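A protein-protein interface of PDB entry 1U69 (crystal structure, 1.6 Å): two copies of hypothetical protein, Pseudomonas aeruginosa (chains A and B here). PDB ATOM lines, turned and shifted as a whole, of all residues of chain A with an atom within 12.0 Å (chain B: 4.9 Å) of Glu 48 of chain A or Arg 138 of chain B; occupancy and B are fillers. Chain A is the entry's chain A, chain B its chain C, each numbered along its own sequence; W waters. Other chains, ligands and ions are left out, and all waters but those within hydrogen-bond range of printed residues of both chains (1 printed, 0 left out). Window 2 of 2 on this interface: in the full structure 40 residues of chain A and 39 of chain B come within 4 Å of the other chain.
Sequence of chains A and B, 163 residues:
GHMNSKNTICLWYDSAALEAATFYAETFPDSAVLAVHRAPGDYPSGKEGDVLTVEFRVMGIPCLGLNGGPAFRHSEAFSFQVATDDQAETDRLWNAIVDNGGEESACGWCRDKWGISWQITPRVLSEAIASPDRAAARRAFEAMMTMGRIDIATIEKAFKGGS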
ATOM      1  N   VAL A  36      19.204 -14.739  -8.424  1.00  0.00           N
ATOM      2  CA  VAL A  36      20.519 -14.110  -8.454  1.00  0.00           C
ATOM      3  C   VAL A  36      20.368 -12.717  -7.877  1.00  0.00           C
ATOM      4  O   VAL A  36      19.461 -11.971  -8.280  1.00  0.00           O
ATOM      5  CB  VAL A  36      21.051 -14.064  -9.885  1.00  0.00           C
ATOM      6  CG1 VAL A  36      22.408 -13.366  -9.959  1.00  0.00           C
ATOM      7  CG2 VAL A  36      21.135 -15.480 -10.433  1.00  0.00           C
ATOM      8  N   HIS A  37      21.226 -12.390  -6.910  1.00  0.00           N
ATOM      9  CA  HIS A  37      21.146 -11.133  -6.172  1.00  0.00           C
ATOM     10  C   HIS A  37      22.421 -10.355  -6.399  1.00  0.00           C
ATOM     11  O   HIS A  37      23.513 -10.817  -6.072  1.00  0.00           O
ATOM     12  CB  HIS A  37      20.968 -11.384  -4.683  1.00  0.00           C
ATOM     13  CG  HIS A  37      19.715 -12.129  -4.352  1.00  0.00           C
ATOM     14  ND1 HIS A  37      18.465 -11.639  -4.660  1.00  0.00           N
ATOM     15  CD2 HIS A  37      19.516 -13.333  -3.767  1.00  0.00           C
ATOM     16  CE1 HIS A  37      17.547 -12.508  -4.274  1.00  0.00           C
ATOM     17  NE2 HIS A  37      18.158 -13.545  -3.727  1.00  0.00           N
ATOM     18  N   ARG A  38      22.284  -9.156  -6.942  1.00  0.00           N
ATOM     19  CA  ARG A  38      23.449  -8.359  -7.265  1.00  0.00           C
ATOM     20  C   ARG A  38      23.802  -7.423  -6.121  1.00  0.00           C
ATOM     21  O   ARG A  38      22.947  -7.071  -5.313  1.00  0.00           O
ATOM     22  CB  ARG A  38      23.239  -7.618  -8.591  1.00  0.00           C
ATOM     23  CG  ARG A  38      23.452  -8.573  -9.760  1.00  0.00           C
ATOM     24  CD  ARG A  38      22.927  -8.129 -11.097  1.00  0.00           C
ATOM     25  NE  ARG A  38      22.950  -9.252 -12.037  1.00  0.00           N
ATOM     26  CZ  ARG A  38      24.045  -9.740 -12.633  1.00  0.00           C
ATOM     27  NH1 ARG A  38      25.247  -9.208 -12.424  1.00  0.00           N
ATOM     28  NH2 ARG A  38      23.938 -10.771 -13.464  1.00  0.00           N
ATOM     29  N   ALA A  39      25.084  -7.072  -6.031  1.00  0.00           N
ATOM     30  CA  ALA A  39      25.601  -6.243  -4.946  1.00  0.00           C
ATOM     31  C   ALA A  39      25.062  -4.826  -5.105  1.00  0.00           C
ATOM     32  O   ALA A  39      25.205  -4.242  -6.178  1.00  0.00           O
ATOM     33  CB  ALA A  39      27.101  -6.230  -4.976  1.00  0.00           C
ATOM     34  N   PRO A  40      24.425  -4.277  -4.070  1.00  0.00           N
ATOM     35  CA  PRO A  40      23.884  -2.914  -4.176  1.00  0.00           C
ATOM     36  C   PRO A  40      24.954  -1.837  -4.059  1.00  0.00           C
ATOM     37  O   PRO A  40      24.674  -0.691  -4.393  1.00  0.00           O
ATOM     38  CB  PRO A  40      22.870  -2.830  -3.026  1.00  0.00           C
ATOM     39  CG  PRO A  40      23.243  -3.892  -2.064  1.00  0.00           C
ATOM     40  CD  PRO A  40      24.108  -4.902  -2.775  1.00  0.00           C
ATOM     41  N   GLY A  41      26.145  -2.201  -3.601  1.00  0.00           N
ATOM     42  CA  GLY A  41      27.277  -1.295  -3.602  1.00  0.00           C
ATOM     43  C   GLY A  41      28.592  -2.026  -3.712  1.00  0.00           C
ATOM     44  O   GLY A  41      28.643  -3.263  -3.663  1.00  0.00           O
ATOM     45  N   ASP A  42      29.667  -1.261  -3.847  1.00  0.00           N
ATOM     46  CA  ASP A  42      31.004  -1.818  -3.848  1.00  0.00           C
ATOM     47  C   ASP A  42      31.265  -2.468  -2.497  1.00  0.00           C
ATOM     48  O   ASP A  42      30.739  -2.038  -1.466  1.00  0.00           O
ATOM     49  CB  ASP A  42      32.049  -0.729  -4.088  1.00  0.00           C
ATOM     50  CG  ASP A  42      31.998  -0.138  -5.491  1.00  0.00           C
ATOM     51  OD1 ASP A  42      31.466  -0.774  -6.431  1.00  0.00           O
ATOM     52  OD2 ASP A  42      32.475   0.988  -5.750  1.00  0.00           O
ATOM     53  N   TYR A  43      32.056  -3.525  -2.510  1.00  0.00           N
ATOM     54  CA  TYR A  43      32.379  -4.240  -1.289  1.00  0.00           C
ATOM     55  C   TYR A  43      33.758  -4.887  -1.451  1.00  0.00           C
ATOM     56  O   TYR A  43      34.364  -4.798  -2.524  1.00  0.00           O
ATOM     57  CB  TYR A  43      31.247  -5.210  -0.927  1.00  0.00           C
ATOM     58  CG  TYR A  43      31.126  -6.453  -1.774  1.00  0.00           C
ATOM     59  CD1 TYR A  43      31.530  -7.688  -1.278  1.00  0.00           C
ATOM     60  CD2 TYR A  43      30.557  -6.408  -3.042  1.00  0.00           C
ATOM     61  CE1 TYR A  43      31.408  -8.845  -2.037  1.00  0.00           C
ATOM     62  CE2 TYR A  43      30.424  -7.562  -3.807  1.00  0.00           C
ATOM     63  CZ  TYR A  43      30.864  -8.777  -3.299  1.00  0.00           C
ATOM     64  OH  TYR A  43      30.738  -9.936  -4.033  1.00  0.00           O
ATOM     65  N   PRO A  44      34.298  -5.472  -0.382  1.00  0.00           N
ATOM     66  CA  PRO A  44      35.656  -6.010  -0.441  1.00  0.00           C
ATOM     67  C   PRO A  44      35.978  -6.893  -1.660  1.00  0.00           C
ATOM     68  O   PRO A  44      37.070  -6.748  -2.194  1.00  0.00           O
ATOM     69  CB  PRO A  44      35.792  -6.779   0.874  1.00  0.00           C
ATOM     70  CG  PRO A  44      34.840  -6.108   1.808  1.00  0.00           C
ATOM     71  CD  PRO A  44      33.711  -5.607   0.963  1.00  0.00           C
ATOM     72  N   SER A  45      35.056  -7.751  -2.106  1.00  0.00           N
ATOM     73  CA  SER A  45      35.334  -8.666  -3.227  1.00  0.00           C
ATOM     74  C   SER A  45      34.398  -8.527  -4.438  1.00  0.00           C
ATOM     75  O   SER A  45      34.157  -9.494  -5.164  1.00  0.00           O
ATOM     76  CB  SER A  45      35.278 -10.112  -2.711  1.00  0.00           C
ATOM     77  OG  SER A  45      33.979 -10.434  -2.236  1.00  0.00           O
ATOM     78  N   GLY A  46      33.857  -7.339  -4.664  1.00  0.00           N
ATOM     79  CA  GLY A  46      33.063  -7.113  -5.850  1.00  0.00           C
ATOM     80  C   GLY A  46      32.635  -5.670  -6.006  1.00  0.00           C
ATOM     81  O   GLY A  46      32.651  -4.897  -5.049  1.00  0.00           O
ATOM     82  N   LYS A  47      32.252  -5.324  -7.226  1.00  0.00           N
ATOM     83  CA  LYS A  47      31.711  -4.011  -7.530  1.00  0.00           C
ATOM     84  C   LYS A  47      30.197  -4.046  -7.422  1.00  0.00           C
ATOM     85  O   LYS A  47      29.568  -5.099  -7.517  1.00  0.00           O
ATOM     86  CB  LYS A  47      32.089  -3.581  -8.946  1.00  0.00           C
ATOM     87  CG  LYS A  47      33.569  -3.598  -9.211  1.00  0.00           C
ATOM     88  CD  LYS A  47      33.918  -2.950 -10.532  1.00  0.00           C
ATOM     89  CE  LYS A  47      35.429  -2.726 -10.626  1.00  0.00           C
ATOM     90  NZ  LYS A  47      35.880  -2.310 -11.987  1.00  0.00           N
ATOM     91  N   GLU A  48      29.602  -2.875  -7.250  1.00  0.00           N
ATOM     92  CA  GLU A  48      28.166  -2.738  -7.363  1.00  0.00           C
ATOM     93  C   GLU A  48      27.712  -3.353  -8.683  1.00  0.00           C
ATOM     94  O   GLU A  48      28.309  -3.095  -9.732  1.00  0.00           O
ATOM     95  CB  GLU A  48      27.763  -1.257  -7.316  1.00  0.00           C
ATOM     96  CG  GLU A  48      26.279  -1.039  -7.527  1.00  0.00           C
ATOM     97  CD  GLU A  48      25.852   0.410  -7.415  1.00  0.00           C
ATOM     98  OE1 GLU A  48      26.654   1.238  -6.941  1.00  0.00           O
ATOM     99  OE2 GLU A  48      24.702   0.704  -7.786  1.00  0.00           O
ATOM    100  N   GLY A  49      26.681  -4.189  -8.619  1.00  0.00           N
ATOM    101  CA  GLY A  49      26.101  -4.805  -9.798  1.00  0.00           C
ATOM    102  C   GLY A  49      26.652  -6.190 -10.094  1.00  0.00           C
ATOM    103  O   GLY A  49      26.095  -6.898 -10.909  1.00  0.00           O
ATOM    104  N   ASP A  50      27.750  -6.570  -9.445  1.00  0.00           N
ATOM    105  CA  ASP A  50      28.300  -7.925  -9.562  1.00  0.00           C
ATOM    106  C   ASP A  50      27.370  -8.882  -8.835  1.00  0.00           C
ATOM    107  O   ASP A  50      26.575  -8.456  -8.005  1.00  0.00           O
ATOM    108  CB  ASP A  50      29.711  -8.002  -8.954  1.00  0.00           C
ATOM    109  CG  ASP A  50      30.779  -7.382  -9.843  1.00  0.00           C
ATOM    110  OD1 ASP A  50      30.509  -7.025 -11.008  1.00  0.00           O
ATOM    111  OD2 ASP A  50      31.935  -7.223  -9.454  1.00  0.00           O
ATOM    112  N   VAL A  51      27.461 -10.168  -9.147  1.00  0.00           N
ATOM    113  CA  VAL A  51      26.690 -11.183  -8.431  1.00  0.00           C
ATOM    114  C   VAL A  51      27.212 -11.277  -6.991  1.00  0.00           C
ATOM    115  O   VAL A  51      28.406 -11.508  -6.761  1.00  0.00           O
ATOM    116  CB  VAL A  51      26.776 -12.564  -9.118  1.00  0.00           C
ATOM    117  CG1 VAL A  51      26.100 -13.652  -8.253  1.00  0.00           C
ATOM    118  CG2 VAL A  51      26.158 -12.523 -10.518  1.00  0.00           C
ATOM    119  N   LEU A  52      26.326 -11.048  -6.028  1.00  0.00           N
ATOM    120  CA  LEU A  52      26.689 -11.121  -4.616  1.00  0.00           C
ATOM    121  C   LEU A  52      26.300 -12.484  -4.039  1.00  0.00           C
ATOM    122  O   LEU A  52      27.138 -13.179  -3.454  1.00  0.00           O
ATOM    123  CB  LEU A  52      26.032  -9.983  -3.830  1.00  0.00           C
ATOM    124  CG  LEU A  52      26.263  -9.938  -2.322  1.00  0.00           C
ATOM    125  CD1 LEU A  52      27.733  -9.790  -2.030  1.00  0.00           C
ATOM    126  CD2 LEU A  52      25.473  -8.807  -1.691  1.00  0.00           C
ATOM    127  N   THR A  53      25.032 -12.858  -4.184  1.00  0.00           N
ATOM    128  CA  THR A  53      24.593 -14.208  -3.813  1.00  0.00           C
ATOM    129  C   THR A  53      23.733 -14.848  -4.886  1.00  0.00           C
ATOM    130  O   THR A  53      23.120 -14.175  -5.720  1.00  0.00           O
ATOM    131  CB  THR A  53      23.804 -14.239  -2.493  1.00  0.00           C
ATOM    132  OG1 THR A  53      22.616 -13.430  -2.599  1.00  0.00           O
ATOM    133  CG2 THR A  53      24.608 -13.681  -1.329  1.00  0.00           C
ATOM    134  N   ASN A  67      29.525 -14.817  -3.115  1.00  0.00           N
ATOM    135  CA  ASN A  67      30.780 -14.342  -3.691  1.00  0.00           C
ATOM    136  C   ASN A  67      31.526 -13.445  -2.710  1.00  0.00           C
ATOM    137  O   ASN A  67      31.368 -12.228  -2.702  1.00  0.00           O
ATOM    138  CB  ASN A  67      30.524 -13.629  -5.021  1.00  0.00           C
ATOM    139  CG  ASN A  67      30.193 -14.605  -6.138  1.00  0.00           C
ATOM    140  OD1 ASN A  67      30.689 -15.736  -6.136  1.00  0.00           O
ATOM    141  ND2 ASN A  67      29.355 -14.185  -7.089  1.00  0.00           N
ATOM    142  N   ARG B 134      17.501   0.404  -5.453  1.00  0.00           N
ATOM    143  CA  ARG B 134      18.959   0.297  -5.302  1.00  0.00           C
ATOM    144  C   ARG B 134      19.536   1.236  -4.235  1.00  0.00           C
ATOM    145  O   ARG B 134      20.448   0.855  -3.499  1.00  0.00           O
ATOM    146  CB  ARG B 134      19.628   0.559  -6.665  1.00  0.00           C
ATOM    147  CG  ARG B 134      21.165   0.654  -6.665  1.00  0.00           C
ATOM    148  CD  ARG B 134      21.897  -0.552  -6.082  1.00  0.00           C
ATOM    149  NE  ARG B 134      21.522  -1.823  -6.709  1.00  0.00           N
ATOM    150  CZ  ARG B 134      22.122  -2.379  -7.765  1.00  0.00           C
ATOM    151  NH1 ARG B 134      23.138  -1.788  -8.377  1.00  0.00           N
ATOM    152  NH2 ARG B 134      21.683  -3.547  -8.223  1.00  0.00           N
ATOM    153  N   ALA B 135      19.031   2.465  -4.170  1.00  0.00           N
ATOM    154  CA  ALA B 135      19.495   3.433  -3.178  1.00  0.00           C
ATOM    155  C   ALA B 135      19.212   2.945  -1.758  1.00  0.00           C
ATOM    156  O   ALA B 135      20.083   3.019  -0.899  1.00  0.00           O
ATOM    157  CB  ALA B 135      18.834   4.774  -3.395  1.00  0.00           C
ATOM    158  N   ALA B 136      17.991   2.461  -1.525  1.00  0.00           N
ATOM    159  CA  ALA B 136      17.586   1.943  -0.213  1.00  0.00           C
ATOM    160  C   ALA B 136      18.377   0.682   0.140  1.00  0.00           C
ATOM    161  O   ALA B 136      18.854   0.527   1.265  1.00  0.00           O
ATOM    162  CB  ALA B 136      16.109   1.644  -0.193  1.00  0.00           C
ATOM    163  N   ALA B 137      18.519  -0.199  -0.842  1.00  0.00           N
ATOM    164  CA  ALA B 137      19.274  -1.441  -0.671  1.00  0.00           C
ATOM    165  C   ALA B 137      20.708  -1.134  -0.267  1.00  0.00           C
ATOM    166  O   ALA B 137      21.255  -1.778   0.617  1.00  0.00           O
ATOM    167  CB  ALA B 137      19.250  -2.254  -1.954  1.00  0.00           C
ATOM    168  N   ARG B 138      21.313  -0.140  -0.913  1.00  0.00           N
ATOM    169  CA  ARG B 138      22.682   0.212  -0.609  1.00  0.00           C
ATOM    170  C   ARG B 138      22.806   0.815   0.790  1.00  0.00           C
ATOM    171  O   ARG B 138      23.781   0.553   1.454  1.00  0.00           O
ATOM    172  CB  ARG B 138      23.267   1.169  -1.657  1.00  0.00           C
ATOM    173  CG  ARG B 138      24.779   1.312  -1.545  1.00  0.00           C
ATOM    174  CD  ARG B 138      25.382   2.376  -2.443  1.00  0.00           C
ATOM    175  NE  ARG B 138      24.980   2.197  -3.834  1.00  0.00           N
ATOM    176  CZ  ARG B 138      24.093   2.955  -4.480  1.00  0.00           C
ATOM    177  NH1 ARG B 138      23.491   3.982  -3.884  1.00  0.00           N
ATOM    178  NH2 ARG B 138      23.811   2.681  -5.744  1.00  0.00           N
ATOM    179  N   ARG B 139      21.842   1.626   1.227  1.00  0.00           N
ATOM    180  CA  ARG B 139      21.881   2.185   2.583  1.00  0.00           C
ATOM    181  C   ARG B 139      21.846   1.061   3.618  1.00  0.00           C
ATOM    182  O   ARG B 139      22.604   1.073   4.586  1.00  0.00           O
ATOM    183  CB  ARG B 139      20.718   3.138   2.832  1.00  0.00           C
ATOM    184  CG  ARG B 139      20.776   4.441   2.057  1.00  0.00           C
ATOM    185  CD  ARG B 139      19.743   5.458   2.524  1.00  0.00           C
ATOM    186  NE  ARG B 139      18.365   5.089   2.204  1.00  0.00           N
ATOM    187  CZ  ARG B 139      17.763   5.308   1.040  1.00  0.00           C
ATOM    188  NH1 ARG B 139      18.392   5.919   0.037  1.00  0.00           N
ATOM    189  NH2 ARG B 139      16.506   4.932   0.879  1.00  0.00           N
ATOM    190  N   ALA B 140      21.009   0.063   3.372  1.00  0.00           N
ATOM    191  CA  ALA B 140      20.889  -1.073   4.286  1.00  0.00           C
ATOM    192  C   ALA B 140      22.171  -1.913   4.303  1.00  0.00           C
ATOM    193  O   ALA B 140      22.613  -2.334   5.362  1.00  0.00           O
ATOM    194  CB  ALA B 140      19.689  -1.937   3.913  1.00  0.00           C
ATOM    195  N   PHE B 141      22.754  -2.114   3.121  1.00  0.00           N
ATOM    196  CA  PHE B 141      24.031  -2.812   2.909  1.00  0.00           C
ATOM    197  C   PHE B 141      25.169  -2.123   3.672  1.00  0.00           C
ATOM    198  O   PHE B 141      25.937  -2.774   4.368  1.00  0.00           O
ATOM    199  CB  PHE B 141      24.305  -2.833   1.397  1.00  0.00           C
ATOM    200  CG  PHE B 141      25.384  -3.778   0.945  1.00  0.00           C
ATOM    201  CD1 PHE B 141      25.357  -5.121   1.288  1.00  0.00           C
ATOM    202  CD2 PHE B 141      26.387  -3.334   0.093  1.00  0.00           C
ATOM    203  CE1 PHE B 141      26.330  -5.985   0.826  1.00  0.00           C
ATOM    204  CE2 PHE B 141      27.362  -4.197  -0.375  1.00  0.00           C
ATOM    205  CZ  PHE B 141      27.339  -5.530  -0.001  1.00  0.00           C
ATOM    206  N   GLU B 142      25.260  -0.795   3.567  1.00  0.00           N
ATOM    207  CA  GLU B 142      26.292  -0.040   4.287  1.00  0.00           C
ATOM    208  C   GLU B 142      26.096  -0.074   5.802  1.00  0.00           C
ATOM    209  O   GLU B 142      27.072  -0.198   6.568  1.00  0.00           O
ATOM    210  CB  GLU B 142      26.315   1.414   3.814  1.00  0.00           C
ATOM    211  CG  GLU B 142      26.826   1.574   2.395  1.00  0.00           C
ATOM    212  CD  GLU B 142      26.662   2.990   1.872  1.00  0.00           C
ATOM    213  OE1 GLU B 142      25.520   3.510   1.894  1.00  0.00           O
ATOM    214  OE2 GLU B 142      27.679   3.577   1.439  1.00  0.00           O
HETATM  215  O   HOH W   1      23.086   2.558  -8.774  1.00  0.00           O
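Among the printed residues, merely in contact across the chains: Ala 39 of chain A with Arg 134 of chain B (3.9 Å), Pro 40 of chain A with Arg 134 of chain B (3.3 Å), Pro 40 of chain A with Ala 137 of chain B (3.8 Å), Pro 40 of chain A with Phe 141 of chain B (3.7 Å), Gly 41 of chain A with Phe 141 of chain B (3.7 Å) and Leu 52 of chain A with Phe 141 of chain B (3.9 Å).
O of His 37 of chain A lies within hydrogen-bond range of N of Leu 52 of chain A, at 2.8 Å.
The backbone carbonyl oxygen (O) of Ala 39 of chain A sits at hydrogen-bond distance from the backbone NH (N) of Gly 49 of chain A.
The backbone NH of Ala 39 of chain A is in hydrogen-bond range of the backbone carbonyl oxygen of Asp 50 of chain A (2.8 Å).
The side-chain carboxylate (OD1) of Asp 42 of chain A sits at hydrogen-bond distance from the backbone NH (N) of Glu 48 of chain A, at 2.9 Å.
N of Asn 67 of chain A sits at hydrogen-bond distance from O of Leu 52 of chain A (2.9 Å).
No position is printed for both chains.
Water W1 lies within hydrogen-bond range of OE2 of Glu 48 of chain A (2.7 Å) and NH2 of Arg 138 of chain B (3.1 Å).
O of Pro 40 of chain A lies within hydrogen-bond range of NE of Arg 138 of chain B, 3.0 Å away.
The guanidinium group of Arg 134 of chain B lies within salt-bridge range of the side-chain carboxylate of Glu 48 of chain A.
The side-chain carboxylate (OE2) of Glu 48 of chain A is in salt-bridge range of the guanidinium group (NH2) of Arg 138 of chain B (3.0 Å).
Of chain B, only Arg 134 (3.0 Å) and Arg 138 (3.0 Å) come within 4 Å of Glu 48 of chain A.
Arg 138 of chain B touches just these residues of chain A: Pro 40 and Glu 48.
No residue of chain A comes within 4 Å of Ala 136 of chain B.
Of the printed residues of chain A, Ala 137 of chain B touches Pro 40.
No residue of chain A comes within 4 Å of Arg 139 of chain B.
No residue of chain A comes within 4 Å of Ala 140 of chain B.
No residue of chain A comes within 4 Å of Glu 142 of chain B.
Of the printed residues of chain B, Leu 52 of chain A touches Phe 141 (3.9 Å).
Of the printed residues of chain B, Ala 39 of chain A touches Arg 134 (3.9 Å).
Printed residues of chain B within 4 Å of Pro 40 of chain A: Arg 134 (3.3 Å), Ala 137 (3.8 Å), Arg 138 (3.0 Å) and Phe 141 (3.7 Å).
Of the printed residues of chain B, Gly 41 of chain A touches Phe 141 (3.7 Å).
Asp 42 of chain A touches none of the printed residues of chain B.
Arg 38 of chain A touches none of the printed residues of chain B.
The nearest residue of chain A that does not touch Arg 138 of chain B is Gly 41 of chain A (4.2 Å).
Hydrophobic or aromatic side chains of chain A that line the printed part of chain B: Pro 40 and Leu 52.
Of the 9 printed residues of chain B, 4 touch a printed residue of chain A.
Printed residues of chain B that touch a printed residue of chain A: Arg 134, Ala 137, Arg 138 and Phe 141.
Hydrophobic or aromatic side chains of chain B within 4 Å of the printed part of chain A: Ala 137 and Phe 141.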
